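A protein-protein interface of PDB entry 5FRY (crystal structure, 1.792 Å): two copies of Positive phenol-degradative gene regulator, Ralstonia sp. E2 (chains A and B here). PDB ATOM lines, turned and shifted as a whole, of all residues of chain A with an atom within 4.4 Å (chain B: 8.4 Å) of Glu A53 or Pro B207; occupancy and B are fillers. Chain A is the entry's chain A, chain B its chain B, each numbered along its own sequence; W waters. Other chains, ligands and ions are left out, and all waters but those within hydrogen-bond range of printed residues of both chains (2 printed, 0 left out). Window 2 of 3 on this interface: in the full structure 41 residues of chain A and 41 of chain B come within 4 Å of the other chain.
Water W2 lies within hydrogen-bond range of the side-chain carboxylate (OE2) of Glu A53 and a ring nitrogen (NE2) of His B73. Water W1 lies within hydrogen-bond range of O of Leu B66 and OE2 of Glu A53.
Of the 9 printed residues of chain A, 4 touch a printed residue of chain B. Hydrophobic or aromatic side chains of chain A that line the printed part of chain B: Ala A49, Leu A50 and Leu A54. Among the printed residues, 7 pairs touch across the chains.
Among the printed residues, pairs that only touch across the chains: Ala A49 with His B73, Leu A50 with Leu B66, Leu A50 with Met B70, Glu A53 with Leu B66, Glu A53 with Pro B207 and Leu A54 with Leu B54.
NH1 of Arg B69 is in hydrogen-bond range of O of Leu B204. O of Gln B206 is in hydrogen-bond range of NH1 of Arg B69, at 3.3 Å.
Of chain B, only Leu B66, Arg B69 and Pro B207 come within 4 Å of Glu A53. Pro B207 touches just one residue of chain A: Glu A53 (3.7 Å). Of the printed residues of chain B, Leu A54 touches Leu B54. Of the printed residues of chain A, Leu B66 touches Leu A50 and Glu A53. Asp A56 touches none of the printed residues of chain B. The nearest printed residue of chain A that does not touch Pro B207 is Thr A57 (6.9 Å). The nearest printed residue of chain B that does not touch Leu A54 is Leu B66 (4.04 Å).
Leu B54 touches its own counterpart, Leu A54. Of the 7 pairs that touch across the chains among the printed residues, 1 has its exchanged pair printed and touching as well.
OE2 of Glu A53 lies within salt-bridge range of NE of Arg B69 (2.8 Å).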
ATOM      1  N   ALA A  49       8.395 -19.613 -11.543  1.00  0.00           N
ATOM      2  CA  ALA A  49       8.281 -19.313 -12.974  1.00  0.00           C
ATOM      3  C   ALA A  49       6.877 -19.634 -13.489  1.00  0.00           C
ATOM      4  O   ALA A  49       6.219 -18.787 -14.104  1.00  0.00           O
ATOM      5  CB  ALA A  49       9.328 -20.083 -13.769  1.00  0.00           C
ATOM      6  N   LEU A  50       6.404 -20.851 -13.228  1.00  0.00           N
ATOM      7  CA  LEU A  50       5.061 -21.226 -13.655  1.00  0.00           C
ATOM      8  C   LEU A  50       3.992 -20.347 -13.005  1.00  0.00           C
ATOM      9  O   LEU A  50       2.995 -20.036 -13.635  1.00  0.00           O
ATOM     10  CB  LEU A  50       4.766 -22.693 -13.336  1.00  0.00           C
ATOM     11  CG  LEU A  50       3.320 -23.134 -13.548  1.00  0.00           C
ATOM     12  CD1 LEU A  50       2.931 -23.185 -15.027  1.00  0.00           C
ATOM     13  CD2 LEU A  50       3.068 -24.483 -12.873  1.00  0.00           C
ATOM     14  N   ARG A  51       4.210 -19.953 -11.756  1.00  0.00           N
ATOM     15  CA  ARG A  51       3.259 -19.094 -11.045  1.00  0.00           C
ATOM     16  C   ARG A  51       3.112 -17.744 -11.728  1.00  0.00           C
ATOM     17  O   ARG A  51       2.011 -17.208 -11.852  1.00  0.00           O
ATOM     18  CB  ARG A  51       3.685 -18.859  -9.599  1.00  0.00           C
ATOM     19  CG  ARG A  51       2.813 -17.803  -8.921  1.00  0.00           C
ATOM     20  CD  ARG A  51       3.269 -17.476  -7.525  1.00  0.00           C
ATOM     21  NE  ARG A  51       2.951 -18.569  -6.626  1.00  0.00           N
ATOM     22  CZ  ARG A  51       2.281 -18.447  -5.490  1.00  0.00           C
ATOM     23  NH1 ARG A  51       1.837 -17.259  -5.068  1.00  0.00           N
ATOM     24  NH2 ARG A  51       2.062 -19.532  -4.766  1.00  0.00           N
ATOM     25  N   LYS A  52       4.251 -17.198 -12.141  1.00  0.00           N
ATOM     26  CA  LYS A  52       4.297 -15.933 -12.849  1.00  0.00           C
ATOM     27  C   LYS A  52       3.535 -15.979 -14.166  1.00  0.00           C
ATOM     28  O   LYS A  52       2.753 -15.078 -14.470  1.00  0.00           O
ATOM     29  CB  LYS A  52       5.741 -15.537 -13.108  1.00  0.00           C
ATOM     30  CG  LYS A  52       5.853 -14.257 -13.899  1.00  0.00           C
ATOM     31  CD  LYS A  52       6.862 -13.329 -13.272  1.00  0.00           C
ATOM     32  CE  LYS A  52       7.004 -12.058 -14.085  1.00  0.00           C
ATOM     33  NZ  LYS A  52       8.378 -11.493 -13.918  1.00  0.00           N
ATOM     34  N   GLU A  53       3.761 -17.030 -14.950  1.00  0.00           N
ATOM     35  CA  GLU A  53       3.042 -17.203 -16.206  1.00  0.00           C
ATOM     36  C   GLU A  53       1.545 -17.408 -15.999  1.00  0.00           C
ATOM     37  O   GLU A  53       0.739 -16.903 -16.780  1.00  0.00           O
ATOM     38  CB  GLU A  53       3.619 -18.381 -17.000  1.00  0.00           C
ATOM     39  CG  GLU A  53       5.040 -18.150 -17.512  1.00  0.00           C
ATOM     40  CD  GLU A  53       5.347 -18.968 -18.752  1.00  0.00           C
ATOM     41  OE1 GLU A  53       4.521 -18.956 -19.693  1.00  0.00           O
ATOM     42  OE2 GLU A  53       6.409 -19.632 -18.791  1.00  0.00           O
ATOM     43  N   LEU A  54       1.166 -18.147 -14.959  1.00  0.00           N
ATOM     44  CA  LEU A  54      -0.249 -18.374 -14.697  1.00  0.00           C
ATOM     45  C   LEU A  54      -0.956 -17.097 -14.249  1.00  0.00           C
ATOM     46  O   LEU A  54      -2.110 -16.876 -14.605  1.00  0.00           O
ATOM     47  CB  LEU A  54      -0.448 -19.476 -13.652  1.00  0.00           C
ATOM     48  CG  LEU A  54      -0.157 -20.891 -14.142  1.00  0.00           C
ATOM     49  CD1 LEU A  54      -0.548 -21.887 -13.086  1.00  0.00           C
ATOM     50  CD2 LEU A  54      -0.869 -21.194 -15.458  1.00  0.00           C
ATOM     51  N   VAL A  55      -0.276 -16.258 -13.477  1.00  0.00           N
ATOM     52  CA  VAL A  55      -0.888 -15.007 -13.036  1.00  0.00           C
ATOM     53  C   VAL A  55      -1.021 -14.068 -14.225  1.00  0.00           C
ATOM     54  O   VAL A  55      -2.126 -13.665 -14.598  1.00  0.00           O
ATOM     55  CB  VAL A  55      -0.075 -14.318 -11.920  1.00  0.00           C
ATOM     56  CG1 VAL A  55      -0.631 -12.929 -11.634  1.00  0.00           C
ATOM     57  CG2 VAL A  55      -0.066 -15.174 -10.655  1.00  0.00           C
ATOM     58  N   ASP A  56       0.125 -13.753 -14.824  1.00  0.00           N
ATOM     59  CA  ASP A  56       0.221 -12.902 -16.008  1.00  0.00           C
ATOM     60  C   ASP A  56      -0.785 -13.228 -17.111  1.00  0.00           C
ATOM     61  O   ASP A  56      -1.243 -12.323 -17.812  1.00  0.00           O
ATOM     62  CB  ASP A  56       1.641 -12.974 -16.588  1.00  0.00           C
ATOM     63  CG  ASP A  56       2.661 -12.234 -15.739  1.00  0.00           C
ATOM     64  OD1 ASP A  56       2.266 -11.289 -15.020  1.00  0.00           O
ATOM     65  OD2 ASP A  56       3.863 -12.591 -15.793  1.00  0.00           O
ATOM     66  N   THR A  57      -1.135 -14.499 -17.287  1.00  0.00           N
ATOM     67  CA  THR A  57      -2.069 -14.829 -18.366  1.00  0.00           C
ATOM     68  C   THR A  57      -3.467 -15.218 -17.879  1.00  0.00           C
ATOM     69  O   THR A  57      -4.445 -15.054 -18.612  1.00  0.00           O
ATOM     70  CB  THR A  57      -1.536 -15.969 -19.260  1.00  0.00           C
ATOM     71  OG1 THR A  57      -0.306 -15.576 -19.874  1.00  0.00           O
ATOM     72  CG2 THR A  57      -2.554 -16.349 -20.327  1.00  0.00           C
ATOM     73  N   LEU B  54      -4.805 -27.480 -16.212  1.00  0.00           N
ATOM     74  CA  LEU B  54      -4.288 -26.635 -17.280  1.00  0.00           C
ATOM     75  C   LEU B  54      -4.651 -27.169 -18.670  1.00  0.00           C
ATOM     76  O   LEU B  54      -5.034 -26.396 -19.551  1.00  0.00           O
ATOM     77  CB  LEU B  54      -2.765 -26.485 -17.154  1.00  0.00           C
ATOM     78  CG  LEU B  54      -2.322 -25.682 -15.931  1.00  0.00           C
ATOM     79  CD1 LEU B  54      -0.807 -25.498 -15.885  1.00  0.00           C
ATOM     80  CD2 LEU B  54      -3.016 -24.329 -15.908  1.00  0.00           C
ATOM     81  N   LEU B  58      -6.826 -24.595 -20.692  1.00  0.00           N
ATOM     82  CA  LEU B  58      -5.985 -23.848 -21.624  1.00  0.00           C
ATOM     83  C   LEU B  58      -5.627 -24.640 -22.872  1.00  0.00           C
ATOM     84  O   LEU B  58      -5.055 -24.092 -23.813  1.00  0.00           O
ATOM     85  CB  LEU B  58      -4.689 -23.413 -20.956  1.00  0.00           C
ATOM     86  CG  LEU B  58      -4.720 -22.624 -19.659  1.00  0.00           C
ATOM     87  CD1 LEU B  58      -3.358 -21.971 -19.494  1.00  0.00           C
ATOM     88  CD2 LEU B  58      -5.821 -21.590 -19.679  1.00  0.00           C
ATOM     89  N   ARG B  62      -0.897 -25.633 -25.051  1.00  0.00           N
ATOM     90  CA  ARG B  62      -0.499 -24.520 -24.190  1.00  0.00           C
ATOM     91  C   ARG B  62      -0.014 -25.028 -22.842  1.00  0.00           C
ATOM     92  O   ARG B  62       0.934 -24.485 -22.277  1.00  0.00           O
ATOM     93  CB  ARG B  62      -1.652 -23.537 -23.992  1.00  0.00           C
ATOM     94  CG  ARG B  62      -1.843 -22.590 -25.161  1.00  0.00           C
ATOM     95  CD  ARG B  62      -3.136 -21.806 -25.042  1.00  0.00           C
ATOM     96  NE  ARG B  62      -3.634 -21.403 -26.358  1.00  0.00           N
ATOM     97  CZ  ARG B  62      -4.872 -20.977 -26.595  1.00  0.00           C
ATOM     98  NH1 ARG B  62      -5.747 -20.895 -25.598  1.00  0.00           N
ATOM     99  NH2 ARG B  62      -5.236 -20.639 -27.828  1.00  0.00           N
ATOM    100  N   GLY B  65       3.592 -26.091 -23.153  1.00  0.00           N
ATOM    101  CA  GLY B  65       4.596 -25.043 -23.159  1.00  0.00           C
ATOM    102  C   GLY B  65       4.910 -24.630 -21.736  1.00  0.00           C
ATOM    103  O   GLY B  65       6.073 -24.522 -21.361  1.00  0.00           O
ATOM    104  N   LEU B  66       3.865 -24.407 -20.940  1.00  0.00           N
ATOM    105  CA  LEU B  66       4.032 -24.080 -19.522  1.00  0.00           C
ATOM    106  C   LEU B  66       4.941 -25.094 -18.810  1.00  0.00           C
ATOM    107  O   LEU B  66       5.835 -24.720 -18.055  1.00  0.00           O
ATOM    108  CB  LEU B  66       2.662 -24.013 -18.835  1.00  0.00           C
ATOM    109  CG  LEU B  66       1.722 -22.930 -19.371  1.00  0.00           C
ATOM    110  CD1 LEU B  66       0.305 -23.090 -18.826  1.00  0.00           C
ATOM    111  CD2 LEU B  66       2.283 -21.555 -19.049  1.00  0.00           C
ATOM    112  N   PHE B  67       4.721 -26.383 -19.058  1.00  0.00           N
ATOM    113  CA  PHE B  67       5.512 -27.388 -18.372  1.00  0.00           C
ATOM    114  C   PHE B  67       6.939 -27.483 -18.896  1.00  0.00           C
ATOM    115  O   PHE B  67       7.853 -27.598 -18.092  1.00  0.00           O
ATOM    116  CB  PHE B  67       4.821 -28.746 -18.425  1.00  0.00           C
ATOM    117  CG  PHE B  67       3.816 -28.917 -17.333  1.00  0.00           C
ATOM    118  CD1 PHE B  67       4.233 -29.189 -16.040  1.00  0.00           C
ATOM    119  CD2 PHE B  67       2.466 -28.730 -17.575  1.00  0.00           C
ATOM    120  CE1 PHE B  67       3.314 -29.318 -15.014  1.00  0.00           C
ATOM    121  CE2 PHE B  67       1.543 -28.861 -16.559  1.00  0.00           C
ATOM    122  CZ  PHE B  67       1.974 -29.145 -15.268  1.00  0.00           C
ATOM    123  N   MET B  68       7.124 -27.445 -20.217  1.00  0.00           N
ATOM    124  CA  MET B  68       8.471 -27.466 -20.813  1.00  0.00           C
ATOM    125  C   MET B  68       9.314 -26.322 -20.292  1.00  0.00           C
ATOM    126  O   MET B  68      10.529 -26.473 -20.057  1.00  0.00           O
ATOM    127  CB  MET B  68       8.408 -27.383 -22.342  1.00  0.00           C
ATOM    128  CG  MET B  68       8.007 -28.656 -23.024  1.00  0.00           C
ATOM    129  SD  MET B  68       7.684 -28.369 -24.764  1.00  0.00           S
ATOM    130  CE  MET B  68       9.349 -28.096 -25.389  1.00  0.00           C
ATOM    131  N   ARG B  69       8.664 -25.173 -20.127  1.00  0.00           N
ATOM    132  CA  ARG B  69       9.334 -23.965 -19.667  1.00  0.00           C
ATOM    133  C   ARG B  69       9.701 -24.102 -18.196  1.00  0.00           C
ATOM    134  O   ARG B  69      10.769 -23.687 -17.798  1.00  0.00           O
ATOM    135  CB  ARG B  69       8.466 -22.725 -19.897  1.00  0.00           C
ATOM    136  CG  ARG B  69       8.519 -22.163 -21.330  1.00  0.00           C
ATOM    137  CD  ARG B  69       7.755 -20.838 -21.453  1.00  0.00           C
ATOM    138  NE  ARG B  69       6.317 -20.987 -21.231  1.00  0.00           N
ATOM    139  CZ  ARG B  69       5.446 -21.309 -22.183  1.00  0.00           C
ATOM    140  NH1 ARG B  69       5.866 -21.527 -23.423  1.00  0.00           N
ATOM    141  NH2 ARG B  69       4.152 -21.420 -21.900  1.00  0.00           N
ATOM    142  N   MET B  70       8.818 -24.702 -17.400  1.00  0.00           N
ATOM    143  CA  MET B  70       9.099 -24.930 -15.984  1.00  0.00           C
ATOM    144  C   MET B  70      10.325 -25.843 -15.813  1.00  0.00           C
ATOM    145  O   MET B  70      11.210 -25.601 -14.989  1.00  0.00           O
ATOM    146  CB  MET B  70       7.865 -25.547 -15.328  1.00  0.00           C
ATOM    147  CG  MET B  70       7.896 -25.574 -13.841  1.00  0.00           C
ATOM    148  SD  MET B  70       6.388 -26.252 -13.201  1.00  0.00           S
ATOM    149  CE  MET B  70       6.267 -25.282 -11.707  1.00  0.00           C
ATOM    150  N   HIS B  73      13.639 -24.058 -16.637  1.00  0.00           N
ATOM    151  CA  HIS B  73      14.173 -23.248 -15.547  1.00  0.00           C
ATOM    152  C   HIS B  73      14.838 -24.125 -14.501  1.00  0.00           C
ATOM    153  O   HIS B  73      15.879 -23.764 -13.973  1.00  0.00           O
ATOM    154  CB  HIS B  73      13.068 -22.386 -14.908  1.00  0.00           C
ATOM    155  CG  HIS B  73      12.560 -21.288 -15.785  1.00  0.00           C
ATOM    156  ND1 HIS B  73      13.251 -20.101 -15.973  1.00  0.00           N
ATOM    157  CD2 HIS B  73      11.426 -21.171 -16.517  1.00  0.00           C
ATOM    158  CE1 HIS B  73      12.570 -19.320 -16.785  1.00  0.00           C
ATOM    159  NE2 HIS B  73      11.459 -19.949 -17.141  1.00  0.00           N
ATOM    160  N   LEU B 202      12.011 -24.204 -30.690  1.00  0.00           N
ATOM    161  CA  LEU B 202      12.610 -23.135 -29.898  1.00  0.00           C
ATOM    162  C   LEU B 202      11.572 -22.120 -29.425  1.00  0.00           C
ATOM    163  O   LEU B 202      11.723 -21.492 -28.370  1.00  0.00           O
ATOM    164  CB  LEU B 202      13.693 -22.438 -30.725  1.00  0.00           C
ATOM    165  CG  LEU B 202      14.212 -21.091 -30.222  1.00  0.00           C
ATOM    166  CD1 LEU B 202      14.846 -21.253 -28.851  1.00  0.00           C
ATOM    167  CD2 LEU B 202      15.196 -20.474 -31.209  1.00  0.00           C
ATOM    168  N   ALA B 203      10.523 -21.960 -30.225  1.00  0.00           N
ATOM    169  CA  ALA B 203       9.418 -21.064 -29.902  1.00  0.00           C
ATOM    170  C   ALA B 203       8.694 -21.490 -28.622  1.00  0.00           C
ATOM    171  O   ALA B 203       8.344 -20.652 -27.783  1.00  0.00           O
ATOM    172  CB  ALA B 203       8.439 -21.006 -31.063  1.00  0.00           C
ATOM    173  N   LEU B 204       8.473 -22.794 -28.475  1.00  0.00           N
ATOM    174  CA  LEU B 204       7.773 -23.332 -27.305  1.00  0.00           C
ATOM    175  C   LEU B 204       8.391 -22.867 -25.978  1.00  0.00           C
ATOM    176  O   LEU B 204       7.700 -22.834 -24.947  1.00  0.00           O
ATOM    177  CB  LEU B 204       7.746 -24.873 -27.341  1.00  0.00           C
ATOM    178  CG  LEU B 204       7.517 -25.644 -28.655  1.00  0.00           C
ATOM    179  CD1 LEU B 204       7.124 -27.094 -28.376  1.00  0.00           C
ATOM    180  CD2 LEU B 204       6.469 -24.974 -29.537  1.00  0.00           C
ATOM    181  N   TYR B 205       9.676 -22.497 -25.991  1.00  0.00           N
ATOM    182  CA  TYR B 205      10.384 -22.146 -24.749  1.00  0.00           C
ATOM    183  C   TYR B 205      10.291 -20.665 -24.382  1.00  0.00           C
ATOM    184  O   TYR B 205      11.023 -20.181 -23.514  1.00  0.00           O
ATOM    185  CB  TYR B 205      11.862 -22.558 -24.837  1.00  0.00           C
ATOM    186  CG  TYR B 205      12.048 -24.058 -24.730  1.00  0.00           C
ATOM    187  CD1 TYR B 205      12.191 -24.670 -23.490  1.00  0.00           C
ATOM    188  CD2 TYR B 205      12.053 -24.861 -25.858  1.00  0.00           C
ATOM    189  CE1 TYR B 205      12.348 -26.038 -23.377  1.00  0.00           C
ATOM    190  CE2 TYR B 205      12.201 -26.250 -25.753  1.00  0.00           C
ATOM    191  CZ  TYR B 205      12.347 -26.825 -24.505  1.00  0.00           C
ATOM    192  OH  TYR B 205      12.505 -28.186 -24.375  1.00  0.00           O
ATOM    193  N   GLN B 206       9.378 -19.960 -25.038  1.00  0.00           N
ATOM    194  CA  GLN B 206       9.167 -18.537 -24.796  1.00  0.00           C
ATOM    195  C   GLN B 206       7.754 -18.242 -24.297  1.00  0.00           C
ATOM    196  O   GLN B 206       6.780 -18.720 -24.874  1.00  0.00           O
ATOM    197  CB  GLN B 206       9.424 -17.760 -26.074  1.00  0.00           C
ATOM    198  CG  GLN B 206      10.851 -17.808 -26.522  1.00  0.00           C
ATOM    199  CD  GLN B 206      11.757 -17.228 -25.471  1.00  0.00           C
ATOM    200  OE1 GLN B 206      11.430 -16.225 -24.838  1.00  0.00           O
ATOM    201  NE2 GLN B 206      12.899 -17.874 -25.256  1.00  0.00           N
ATOM    202  N   PRO B 207       7.637 -17.436 -23.233  1.00  0.00           N
ATOM    203  CA  PRO B 207       6.303 -17.148 -22.691  1.00  0.00           C
ATOM    204  C   PRO B 207       5.456 -16.311 -23.646  1.00  0.00           C
ATOM    205  O   PRO B 207       4.763 -16.899 -24.479  1.00  0.00           O
ATOM    206  CB  PRO B 207       6.601 -16.372 -21.401  1.00  0.00           C
ATOM    207  CG  PRO B 207       8.065 -16.631 -21.105  1.00  0.00           C
ATOM    208  CD  PRO B 207       8.707 -16.807 -22.442  1.00  0.00           C
HETATM  209  O   HOH W   1       5.977 -22.138 -16.899  1.00  0.00           O
HETATM  210  O   HOH W   2       8.561 -19.197 -17.584  1.00  0.00           O
